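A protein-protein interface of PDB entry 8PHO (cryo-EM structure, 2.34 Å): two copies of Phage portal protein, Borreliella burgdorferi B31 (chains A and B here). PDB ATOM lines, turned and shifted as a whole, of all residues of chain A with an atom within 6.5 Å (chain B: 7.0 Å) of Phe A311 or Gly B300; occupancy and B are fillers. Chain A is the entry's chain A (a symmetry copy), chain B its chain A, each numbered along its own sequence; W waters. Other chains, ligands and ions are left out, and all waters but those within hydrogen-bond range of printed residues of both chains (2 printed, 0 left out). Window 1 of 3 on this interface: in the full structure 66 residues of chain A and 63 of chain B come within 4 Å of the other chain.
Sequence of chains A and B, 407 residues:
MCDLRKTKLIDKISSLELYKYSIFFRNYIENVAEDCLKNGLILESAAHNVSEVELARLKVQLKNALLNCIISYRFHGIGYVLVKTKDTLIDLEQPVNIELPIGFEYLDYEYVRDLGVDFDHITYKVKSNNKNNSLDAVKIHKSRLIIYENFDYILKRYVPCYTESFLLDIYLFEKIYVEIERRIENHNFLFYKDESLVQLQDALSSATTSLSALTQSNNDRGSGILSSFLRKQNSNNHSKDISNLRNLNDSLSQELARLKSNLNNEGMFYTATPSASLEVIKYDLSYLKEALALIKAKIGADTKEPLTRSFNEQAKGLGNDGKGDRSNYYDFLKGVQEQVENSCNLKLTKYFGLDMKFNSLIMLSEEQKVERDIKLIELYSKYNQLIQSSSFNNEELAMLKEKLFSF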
ATOM      1  N   PHE A  24       5.310  22.082  -8.648  1.00  0.00           N
ATOM      2  CA  PHE A  24       4.362  21.094  -9.144  1.00  0.00           C
ATOM      3  C   PHE A  24       4.026  20.094  -8.050  1.00  0.00           C
ATOM      4  O   PHE A  24       2.853  19.784  -7.815  1.00  0.00           O
ATOM      5  CB  PHE A  24       4.951  20.400 -10.372  1.00  0.00           C
ATOM      6  CG  PHE A  24       3.974  19.542 -11.137  1.00  0.00           C
ATOM      7  CD1 PHE A  24       2.910  20.119 -11.811  1.00  0.00           C
ATOM      8  CD2 PHE A  24       4.105  18.162 -11.159  1.00  0.00           C
ATOM      9  CE1 PHE A  24       2.007  19.339 -12.507  1.00  0.00           C
ATOM     10  CE2 PHE A  24       3.194  17.375 -11.842  1.00  0.00           C
ATOM     11  CZ  PHE A  24       2.167  17.970 -12.547  1.00  0.00           C
ATOM     12  N   PHE A 173      10.548  14.763 -14.661  1.00  0.00           N
ATOM     13  CA  PHE A 173       9.872  15.932 -15.207  1.00  0.00           C
ATOM     14  C   PHE A 173      10.673  17.197 -14.928  1.00  0.00           C
ATOM     15  O   PHE A 173      10.818  18.055 -15.807  1.00  0.00           O
ATOM     16  CB  PHE A 173       8.462  16.028 -14.628  1.00  0.00           C
ATOM     17  CG  PHE A 173       7.611  17.116 -15.233  1.00  0.00           C
ATOM     18  CD1 PHE A 173       7.796  17.539 -16.543  1.00  0.00           C
ATOM     19  CD2 PHE A 173       6.683  17.778 -14.452  1.00  0.00           C
ATOM     20  CE1 PHE A 173       7.020  18.562 -17.072  1.00  0.00           C
ATOM     21  CE2 PHE A 173       5.908  18.792 -14.972  1.00  0.00           C
ATOM     22  CZ  PHE A 173       6.068  19.175 -16.283  1.00  0.00           C
ATOM     23  N   LEU A 292       9.098  13.679 -22.269  1.00  0.00           N
ATOM     24  CA  LEU A 292       8.032  14.486 -21.681  1.00  0.00           C
ATOM     25  C   LEU A 292       6.672  13.851 -21.933  1.00  0.00           C
ATOM     26  O   LEU A 292       5.816  13.825 -21.041  1.00  0.00           O
ATOM     27  CB  LEU A 292       8.057  15.909 -22.234  1.00  0.00           C
ATOM     28  CG  LEU A 292       6.934  16.777 -21.643  1.00  0.00           C
ATOM     29  CD1 LEU A 292       6.942  16.804 -20.124  1.00  0.00           C
ATOM     30  CD2 LEU A 292       6.944  18.187 -22.228  1.00  0.00           C
ATOM     31  N   ILE A 295       6.386  10.834 -19.682  1.00  0.00           N
ATOM     32  CA  ILE A 295       6.278  11.232 -18.281  1.00  0.00           C
ATOM     33  C   ILE A 295       4.886  11.774 -17.984  1.00  0.00           C
ATOM     34  O   ILE A 295       4.319  11.522 -16.914  1.00  0.00           O
ATOM     35  CB  ILE A 295       7.373  12.249 -17.910  1.00  0.00           C
ATOM     36  CG1 ILE A 295       8.736  11.563 -17.820  1.00  0.00           C
ATOM     37  CG2 ILE A 295       7.053  12.908 -16.576  1.00  0.00           C
ATOM     38  CD1 ILE A 295       9.890  12.528 -17.946  1.00  0.00           C
ATOM     39  N   LYS A 296       4.311  12.508 -18.938  1.00  0.00           N
ATOM     40  CA  LYS A 296       2.950  13.001 -18.777  1.00  0.00           C
ATOM     41  C   LYS A 296       1.956  11.851 -18.703  1.00  0.00           C
ATOM     42  O   LYS A 296       1.016  11.880 -17.900  1.00  0.00           O
ATOM     43  CB  LYS A 296       2.584  13.944 -19.923  1.00  0.00           C
ATOM     44  CG  LYS A 296       1.258  14.651 -19.705  1.00  0.00           C
ATOM     45  CD  LYS A 296       0.947  15.641 -20.818  1.00  0.00           C
ATOM     46  CE  LYS A 296      -0.367  16.352 -20.561  1.00  0.00           C
ATOM     47  NZ  LYS A 296      -0.788  17.207 -21.707  1.00  0.00           N
ATOM     48  N   ILE A 299       2.356  10.256 -15.231  1.00  0.00           N
ATOM     49  CA  ILE A 299       1.759  11.088 -14.191  1.00  0.00           C
ATOM     50  C   ILE A 299       0.241  10.994 -14.239  1.00  0.00           C
ATOM     51  O   ILE A 299      -0.420  10.900 -13.196  1.00  0.00           O
ATOM     52  CB  ILE A 299       2.240  12.545 -14.327  1.00  0.00           C
ATOM     53  CG1 ILE A 299       3.714  12.678 -13.939  1.00  0.00           C
ATOM     54  CG2 ILE A 299       1.387  13.479 -13.480  1.00  0.00           C
ATOM     55  CD1 ILE A 299       4.295  14.026 -14.308  1.00  0.00           C
ATOM     56  N   PRO A 306      -7.286  16.107 -11.099  1.00  0.00           N
ATOM     57  CA  PRO A 306      -7.365  16.444 -12.532  1.00  0.00           C
ATOM     58  C   PRO A 306      -6.367  17.507 -12.968  1.00  0.00           C
ATOM     59  O   PRO A 306      -5.902  17.478 -14.111  1.00  0.00           O
ATOM     60  CB  PRO A 306      -8.815  16.923 -12.688  1.00  0.00           C
ATOM     61  CG  PRO A 306      -9.184  17.413 -11.315  1.00  0.00           C
ATOM     62  CD  PRO A 306      -8.529  16.433 -10.384  1.00  0.00           C
ATOM     63  N   LEU A 307      -6.031  18.440 -12.083  1.00  0.00           N
ATOM     64  CA  LEU A 307      -5.076  19.509 -12.374  1.00  0.00           C
ATOM     65  C   LEU A 307      -3.656  18.977 -12.550  1.00  0.00           C
ATOM     66  O   LEU A 307      -2.902  19.465 -13.401  1.00  0.00           O
ATOM     67  CB  LEU A 307      -5.114  20.567 -11.271  1.00  0.00           C
ATOM     68  CG  LEU A 307      -6.159  21.674 -11.422  1.00  0.00           C
ATOM     69  CD1 LEU A 307      -7.548  21.124 -11.184  1.00  0.00           C
ATOM     70  CD2 LEU A 307      -5.886  22.788 -10.419  1.00  0.00           C
ATOM     71  N   THR A 308      -3.296  17.938 -11.797  1.00  0.00           N
ATOM     72  CA  THR A 308      -1.954  17.372 -11.872  1.00  0.00           C
ATOM     73  C   THR A 308      -1.777  16.540 -13.138  1.00  0.00           C
ATOM     74  O   THR A 308      -0.736  16.624 -13.800  1.00  0.00           O
ATOM     75  CB  THR A 308      -1.653  16.537 -10.624  1.00  0.00           C
ATOM     76  OG1 THR A 308      -1.678  17.367  -9.457  1.00  0.00           O
ATOM     77  CG2 THR A 308      -0.276  15.898 -10.733  1.00  0.00           C
ATOM     78  N   ARG A 309      -2.798  15.768 -13.500  1.00  0.00           N
ATOM     79  CA  ARG A 309      -2.739  14.891 -14.664  1.00  0.00           C
ATOM     80  C   ARG A 309      -2.648  15.691 -15.959  1.00  0.00           C
ATOM     81  O   ARG A 309      -1.824  15.391 -16.831  1.00  0.00           O
ATOM     82  CB  ARG A 309      -3.960  13.983 -14.699  1.00  0.00           C
ATOM     83  CG  ARG A 309      -4.320  13.272 -13.419  1.00  0.00           C
ATOM     84  CD  ARG A 309      -5.573  12.427 -13.582  1.00  0.00           C
ATOM     85  NE  ARG A 309      -5.383  11.333 -14.526  1.00  0.00           N
ATOM     86  CZ  ARG A 309      -5.785  11.360 -15.789  1.00  0.00           C
ATOM     87  NH1 ARG A 309      -6.433  12.400 -16.285  1.00  0.00           N
ATOM     88  NH2 ARG A 309      -5.508  10.328 -16.578  1.00  0.00           N
ATOM     89  N   SER A 310      -3.487  16.717 -16.093  1.00  0.00           N
ATOM     90  CA  SER A 310      -3.623  17.501 -17.316  1.00  0.00           C
ATOM     91  C   SER A 310      -2.687  18.701 -17.367  1.00  0.00           C
ATOM     92  O   SER A 310      -2.798  19.509 -18.289  1.00  0.00           O
ATOM     93  CB  SER A 310      -5.064  18.001 -17.465  1.00  0.00           C
ATOM     94  OG  SER A 310      -5.385  18.816 -16.348  1.00  0.00           O
ATOM     95  N   PHE A 311      -1.797  18.860 -16.394  1.00  0.00           N
ATOM     96  CA  PHE A 311      -0.902  20.021 -16.319  1.00  0.00           C
ATOM     97  C   PHE A 311      -1.686  21.336 -16.313  1.00  0.00           C
ATOM     98  O   PHE A 311      -1.418  22.249 -17.093  1.00  0.00           O
ATOM     99  CB  PHE A 311       0.127  19.985 -17.457  1.00  0.00           C
ATOM    100  CG  PHE A 311       1.156  18.900 -17.299  1.00  0.00           C
ATOM    101  CD1 PHE A 311       1.270  18.188 -16.117  1.00  0.00           C
ATOM    102  CD2 PHE A 311       2.039  18.620 -18.328  1.00  0.00           C
ATOM    103  CE1 PHE A 311       2.225  17.198 -15.982  1.00  0.00           C
ATOM    104  CE2 PHE A 311       3.034  17.681 -18.172  1.00  0.00           C
ATOM    105  CZ  PHE A 311       3.106  16.944 -17.011  1.00  0.00           C
ATOM    106  N   ASN A 312      -2.684  21.409 -15.434  1.00  0.00           N
ATOM    107  CA  ASN A 312      -3.557  22.571 -15.265  1.00  0.00           C
ATOM    108  C   ASN A 312      -4.394  22.891 -16.504  1.00  0.00           C
ATOM    109  O   ASN A 312      -4.858  24.024 -16.670  1.00  0.00           O
ATOM    110  CB  ASN A 312      -2.777  23.827 -14.849  1.00  0.00           C
ATOM    111  CG  ASN A 312      -2.228  23.733 -13.446  1.00  0.00           C
ATOM    112  OD1 ASN A 312      -2.535  22.799 -12.711  1.00  0.00           O
ATOM    113  ND2 ASN A 312      -1.401  24.699 -13.070  1.00  0.00           N
ATOM    114  N   GLU A 313      -4.615  21.919 -17.386  1.00  0.00           N
ATOM    115  CA  GLU A 313      -5.358  22.154 -18.619  1.00  0.00           C
ATOM    116  C   GLU A 313      -6.830  21.795 -18.496  1.00  0.00           C
ATOM    117  O   GLU A 313      -7.651  22.318 -19.260  1.00  0.00           O
ATOM    118  CB  GLU A 313      -4.746  21.361 -19.785  1.00  0.00           C
ATOM    119  CG  GLU A 313      -3.529  22.031 -20.410  1.00  0.00           C
ATOM    120  CD  GLU A 313      -2.763  21.126 -21.360  1.00  0.00           C
ATOM    121  OE1 GLU A 313      -3.048  19.909 -21.400  1.00  0.00           O
ATOM    122  OE2 GLU A 313      -1.887  21.642 -22.086  1.00  0.00           O
ATOM    123  N   GLN A 314      -7.182  20.930 -17.555  1.00  0.00           N
ATOM    124  CA  GLN A 314      -8.552  20.481 -17.371  1.00  0.00           C
ATOM    125  C   GLN A 314      -9.184  21.141 -16.149  1.00  0.00           C
ATOM    126  O   GLN A 314      -8.505  21.698 -15.285  1.00  0.00           O
ATOM    127  CB  GLN A 314      -8.611  18.959 -17.218  1.00  0.00           C
ATOM    128  CG  GLN A 314      -8.479  18.177 -18.514  1.00  0.00           C
ATOM    129  CD  GLN A 314      -8.417  16.684 -18.260  1.00  0.00           C
ATOM    130  OE1 GLN A 314      -8.454  16.239 -17.114  1.00  0.00           O
ATOM    131  NE2 GLN A 314      -8.297  15.902 -19.326  1.00  0.00           N
ATOM    132  N   PHE B 166      10.345  27.219 -11.267  1.00  0.00           N
ATOM    133  CA  PHE B 166       9.649  28.267 -12.010  1.00  0.00           C
ATOM    134  C   PHE B 166      10.616  29.348 -12.472  1.00  0.00           C
ATOM    135  O   PHE B 166      10.527  29.819 -13.612  1.00  0.00           O
ATOM    136  CB  PHE B 166       8.533  28.872 -11.169  1.00  0.00           C
ATOM    137  CG  PHE B 166       7.555  29.702 -11.946  1.00  0.00           C
ATOM    138  CD1 PHE B 166       6.587  29.102 -12.747  1.00  0.00           C
ATOM    139  CD2 PHE B 166       7.614  31.075 -11.896  1.00  0.00           C
ATOM    140  CE1 PHE B 166       5.697  29.892 -13.459  1.00  0.00           C
ATOM    141  CE2 PHE B 166       6.729  31.864 -12.596  1.00  0.00           C
ATOM    142  CZ  PHE B 166       5.751  31.275 -13.355  1.00  0.00           C
ATOM    143  N   LEU B 294       8.500  22.994 -25.035  1.00  0.00           N
ATOM    144  CA  LEU B 294       8.599  22.329 -23.745  1.00  0.00           C
ATOM    145  C   LEU B 294       8.510  23.325 -22.597  1.00  0.00           C
ATOM    146  O   LEU B 294       7.977  23.009 -21.525  1.00  0.00           O
ATOM    147  CB  LEU B 294       9.914  21.570 -23.672  1.00  0.00           C
ATOM    148  CG  LEU B 294      10.308  20.515 -24.709  1.00  0.00           C
ATOM    149  CD1 LEU B 294      11.668  19.895 -24.485  1.00  0.00           C
ATOM    150  CD2 LEU B 294       9.217  19.446 -24.761  1.00  0.00           C
ATOM    151  N   ILE B 295       9.072  24.521 -22.786  1.00  0.00           N
ATOM    152  CA  ILE B 295       9.038  25.534 -21.735  1.00  0.00           C
ATOM    153  C   ILE B 295       7.618  26.047 -21.531  1.00  0.00           C
ATOM    154  O   ILE B 295       7.189  26.299 -20.398  1.00  0.00           O
ATOM    155  CB  ILE B 295      10.015  26.682 -22.045  1.00  0.00           C
ATOM    156  CG1 ILE B 295      11.460  26.229 -21.842  1.00  0.00           C
ATOM    157  CG2 ILE B 295       9.732  27.877 -21.145  1.00  0.00           C
ATOM    158  CD1 ILE B 295      12.459  27.097 -22.568  1.00  0.00           C
ATOM    159  N   LYS B 296       6.866  26.186 -22.624  1.00  0.00           N
ATOM    160  CA  LYS B 296       5.471  26.593 -22.520  1.00  0.00           C
ATOM    161  C   LYS B 296       4.652  25.549 -21.773  1.00  0.00           C
ATOM    162  O   LYS B 296       3.793  25.890 -20.952  1.00  0.00           O
ATOM    163  CB  LYS B 296       4.881  26.837 -23.907  1.00  0.00           C
ATOM    164  CG  LYS B 296       3.497  27.461 -23.858  1.00  0.00           C
ATOM    165  CD  LYS B 296       2.957  27.765 -25.247  1.00  0.00           C
ATOM    166  CE  LYS B 296       1.588  28.412 -25.167  1.00  0.00           C
ATOM    167  NZ  LYS B 296       0.954  28.576 -26.507  1.00  0.00           N
ATOM    168  N   ALA B 297       4.909  24.271 -22.045  1.00  0.00           N
ATOM    169  CA  ALA B 297       4.207  23.203 -21.347  1.00  0.00           C
ATOM    170  C   ALA B 297       4.534  23.231 -19.862  1.00  0.00           C
ATOM    171  O   ALA B 297       3.632  23.129 -19.024  1.00  0.00           O
ATOM    172  CB  ALA B 297       4.556  21.850 -21.963  1.00  0.00           C
ATOM    173  N   LYS B 298       5.806  23.452 -19.521  1.00  0.00           N
ATOM    174  CA  LYS B 298       6.201  23.494 -18.117  1.00  0.00           C
ATOM    175  C   LYS B 298       5.583  24.691 -17.405  1.00  0.00           C
ATOM    176  O   LYS B 298       5.104  24.561 -16.274  1.00  0.00           O
ATOM    177  CB  LYS B 298       7.719  23.536 -17.999  1.00  0.00           C
ATOM    178  CG  LYS B 298       8.234  23.550 -16.578  1.00  0.00           C
ATOM    179  CD  LYS B 298       7.977  22.227 -15.872  1.00  0.00           C
ATOM    180  CE  LYS B 298       8.726  22.190 -14.553  1.00  0.00           C
ATOM    181  NZ  LYS B 298       8.492  20.898 -13.844  1.00  0.00           N
ATOM    182  N   ILE B 299       5.573  25.857 -18.056  1.00  0.00           N
ATOM    183  CA  ILE B 299       4.967  27.040 -17.454  1.00  0.00           C
ATOM    184  C   ILE B 299       3.477  26.821 -17.234  1.00  0.00           C
ATOM    185  O   ILE B 299       2.932  27.191 -16.186  1.00  0.00           O
ATOM    186  CB  ILE B 299       5.234  28.283 -18.325  1.00  0.00           C
ATOM    187  CG1 ILE B 299       6.705  28.696 -18.260  1.00  0.00           C
ATOM    188  CG2 ILE B 299       4.344  29.442 -17.901  1.00  0.00           C
ATOM    189  CD1 ILE B 299       7.065  29.739 -19.295  1.00  0.00           C
ATOM    190  N   GLY B 300       2.795  26.214 -18.207  1.00  0.00           N
ATOM    191  CA  GLY B 300       1.389  25.922 -18.011  1.00  0.00           C
ATOM    192  C   GLY B 300       1.154  24.932 -16.892  1.00  0.00           C
ATOM    193  O   GLY B 300       0.124  24.989 -16.212  1.00  0.00           O
ATOM    194  N   ALA B 301       2.105  24.028 -16.664  1.00  0.00           N
ATOM    195  CA  ALA B 301       1.938  23.081 -15.577  1.00  0.00           C
ATOM    196  C   ALA B 301       2.268  23.669 -14.212  1.00  0.00           C
ATOM    197  O   ALA B 301       1.773  23.139 -13.213  1.00  0.00           O
ATOM    198  CB  ALA B 301       2.812  21.848 -15.815  1.00  0.00           C
ATOM    199  N   ASP B 302       3.051  24.742 -14.149  1.00  0.00           N
ATOM    200  CA  ASP B 302       3.582  25.225 -12.881  1.00  0.00           C
ATOM    201  C   ASP B 302       2.752  26.351 -12.284  1.00  0.00           C
ATOM    202  O   ASP B 302       3.066  26.814 -11.182  1.00  0.00           O
ATOM    203  CB  ASP B 302       5.027  25.703 -13.053  1.00  0.00           C
ATOM    204  CG  ASP B 302       6.024  24.564 -13.067  1.00  0.00           C
ATOM    205  OD1 ASP B 302       5.599  23.393 -12.976  1.00  0.00           O
ATOM    206  OD2 ASP B 302       7.240  24.845 -13.098  1.00  0.00           O
ATOM    207  N   THR B 303       1.734  26.833 -12.991  1.00  0.00           N
ATOM    208  CA  THR B 303       0.934  27.939 -12.492  1.00  0.00           C
ATOM    209  C   THR B 303      -0.497  27.795 -12.985  1.00  0.00           C
ATOM    210  O   THR B 303      -0.781  27.055 -13.929  1.00  0.00           O
ATOM    211  CB  THR B 303       1.478  29.309 -12.925  1.00  0.00           C
ATOM    212  OG1 THR B 303       0.717  30.330 -12.264  1.00  0.00           O
ATOM    213  CG2 THR B 303       1.339  29.475 -14.430  1.00  0.00           C
ATOM    214  N   LYS B 304      -1.399  28.507 -12.315  1.00  0.00           N
ATOM    215  CA  LYS B 304      -2.821  28.472 -12.608  1.00  0.00           C
ATOM    216  C   LYS B 304      -3.348  29.776 -13.190  1.00  0.00           C
ATOM    217  O   LYS B 304      -4.538  29.855 -13.509  1.00  0.00           O
ATOM    218  CB  LYS B 304      -3.605  28.147 -11.332  1.00  0.00           C
ATOM    219  CG  LYS B 304      -3.610  26.693 -10.884  1.00  0.00           C
ATOM    220  CD  LYS B 304      -4.058  26.576  -9.434  1.00  0.00           C
ATOM    221  CE  LYS B 304      -3.778  25.194  -8.876  1.00  0.00           C
ATOM    222  NZ  LYS B 304      -4.049  25.111  -7.416  1.00  0.00           N
ATOM    223  N   THR B 308      -0.724  33.798 -17.850  1.00  0.00           N
ATOM    224  CA  THR B 308       0.670  33.367 -17.842  1.00  0.00           C
ATOM    225  C   THR B 308       0.841  32.044 -18.582  1.00  0.00           C
ATOM    226  O   THR B 308       1.797  31.876 -19.348  1.00  0.00           O
ATOM    227  CB  THR B 308       1.191  33.261 -16.407  1.00  0.00           C
ATOM    228  OG1 THR B 308       1.161  34.546 -15.775  1.00  0.00           O
ATOM    229  CG2 THR B 308       2.626  32.753 -16.400  1.00  0.00           C
ATOM    230  N   ARG B 309      -0.095  31.120 -18.390  1.00  0.00           N
ATOM    231  CA  ARG B 309      -0.024  29.798 -19.003  1.00  0.00           C
ATOM    232  C   ARG B 309      -0.159  29.880 -20.519  1.00  0.00           C
ATOM    233  O   ARG B 309       0.616  29.260 -21.258  1.00  0.00           O
ATOM    234  CB  ARG B 309      -1.111  28.897 -18.432  1.00  0.00           C
ATOM    235  CG  ARG B 309      -1.255  28.865 -16.931  1.00  0.00           C
ATOM    236  CD  ARG B 309      -2.394  27.955 -16.499  1.00  0.00           C
ATOM    237  NE  ARG B 309      -2.144  26.560 -16.837  1.00  0.00           N
ATOM    238  CZ  ARG B 309      -2.658  25.945 -17.892  1.00  0.00           C
ATOM    239  NH1 ARG B 309      -3.482  26.566 -18.719  1.00  0.00           N
ATOM    240  NH2 ARG B 309      -2.318  24.685 -18.138  1.00  0.00           N
ATOM    241  N   SER B 310      -1.137  30.648 -20.997  1.00  0.00           N
ATOM    242  CA  SER B 310      -1.486  30.734 -22.411  1.00  0.00           C
ATOM    243  C   SER B 310      -0.728  31.829 -23.151  1.00  0.00           C
ATOM    244  O   SER B 310      -1.029  32.081 -24.317  1.00  0.00           O
ATOM    245  CB  SER B 310      -2.989  30.993 -22.568  1.00  0.00           C
ATOM    246  OG  SER B 310      -3.314  32.218 -21.929  1.00  0.00           O
ATOM    247  N   PHE B 311       0.217  32.502 -22.504  1.00  0.00           N
ATOM    248  CA  PHE B 311       0.951  33.618 -23.111  1.00  0.00           C
ATOM    249  C   PHE B 311       0.002  34.711 -23.610  1.00  0.00           C
ATOM    250  O   PHE B 311       0.073  35.154 -24.755  1.00  0.00           O
ATOM    251  CB  PHE B 311       1.869  33.116 -24.234  1.00  0.00           C
ATOM    252  CG  PHE B 311       3.044  32.322 -23.736  1.00  0.00           C
ATOM    253  CD1 PHE B 311       3.359  32.278 -22.389  1.00  0.00           C
ATOM    254  CD2 PHE B 311       3.859  31.648 -24.628  1.00  0.00           C
ATOM    255  CE1 PHE B 311       4.446  31.549 -21.943  1.00  0.00           C
ATOM    256  CE2 PHE B 311       4.981  30.976 -24.196  1.00  0.00           C
ATOM    257  CZ  PHE B 311       5.257  30.897 -22.848  1.00  0.00           C
HETATM  258  O   HOH W   1       0.704  22.843 -19.612  1.00  0.00           O
HETATM  259  O   HOH W   2       7.716  22.581 -10.831  1.00  0.00           O
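NH2 of Arg B309 sits at hydrogen-bond distance from O of Phe A311.
O of Phe A311 lies close to O of Gly B300 (3.3 Å).
The guanidinium group (NH2) of Arg B309 sits at hydrogen-bond distance from the backbone carbonyl oxygen (O) of Asn A312 (3.0 Å).
The side-chain amide nitrogen (ND2) of Asn A312 is in hydrogen-bond range of the backbone carbonyl oxygen (O) of Thr B303, 2.6 Å away.
N of Glu A313 sits at hydrogen-bond distance from OG of Ser A310 (3.4 Å).
NE of Arg B309 lies close to O of Thr B303 (3.2 Å).
The side-chain carboxylate of Asp B302 lies within salt-bridge range of the side-chain amino group of Lys B298 (3.9 Å).
NZ of Lys A296 lies within salt-bridge range of OE1 of Glu A313, at 3.5 Å.
The guanidinium group of Arg B309 lies within hydrogen-bond range of the backbone carbonyl oxygen of Gly B300 (2.8 Å).
The backbone carbonyl oxygen of Leu A307 is in hydrogen-bond range of the backbone NH of Asn A312 (2.8 Å).
Among the printed residues, merely in contact across the chains: Asn A312 with Gly B300 (3.4 Å), Phe A24 with Ala B301 (3.5 Å), Phe A173 with Lys B298 (3.5 Å), Asn A312 with Ala B301 (3.5 Å), Leu A307 with Lys B304 (3.6 Å), Leu A292 with Leu B294 (3.6 Å), Phe A311 with Ala B301 (3.7 Å), Glu A313 with Arg B309 (3.7 Å) and Asn A312 with Lys B304 (3.7 Å).
Of the printed residues of chain B, Phe A311 touches Gly B300, Ala B301 and Arg B309.
Gly B300 touches just these residues of chain A: Phe A311 and Asn A312.
Of the printed residues of chain A, Arg B309 touches Phe A311 (2.8 Å), Asn A312 (3.0 Å) and Glu A313 (3.7 Å).
Of the printed residues of chain A, Leu B294 touches Leu A292.
Printed residues of chain A within 4 Å of Lys B298: Phe A173 (3.5 Å).
Asp B302 touches none of the printed residues of chain A.
Along chain B the printed residues that touch a printed residue of chain A span positions 294 to 309.
Printed residues of chain A that touch a printed residue of chain B: Phe A24, Phe A173, Leu A292, Leu A307, Phe A311, Asn A312 and Glu A313.
Hydrophobic or aromatic side chains of chain A that line the printed part of chain B: Phe A24, Phe A173, Leu A292, Leu A307 and Phe A311.
Phe A311 touches Arg B309, but with the chains exchanged Arg A309 does not touch Phe B311 (18.1 Å).
Water W1 lies within hydrogen-bond range of the backbone carbonyl oxygen of Ala B297 (3.0 Å), the backbone carbonyl oxygen of Phe A311 (3.3 Å) and the backbone NH of Ala B301 (3.5 Å).
Water W2 bridges the side-chain carboxylate (OD1) of Asp B302 (3.1 Å) and the backbone NH (N) of Phe A24 (3.3 Å).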
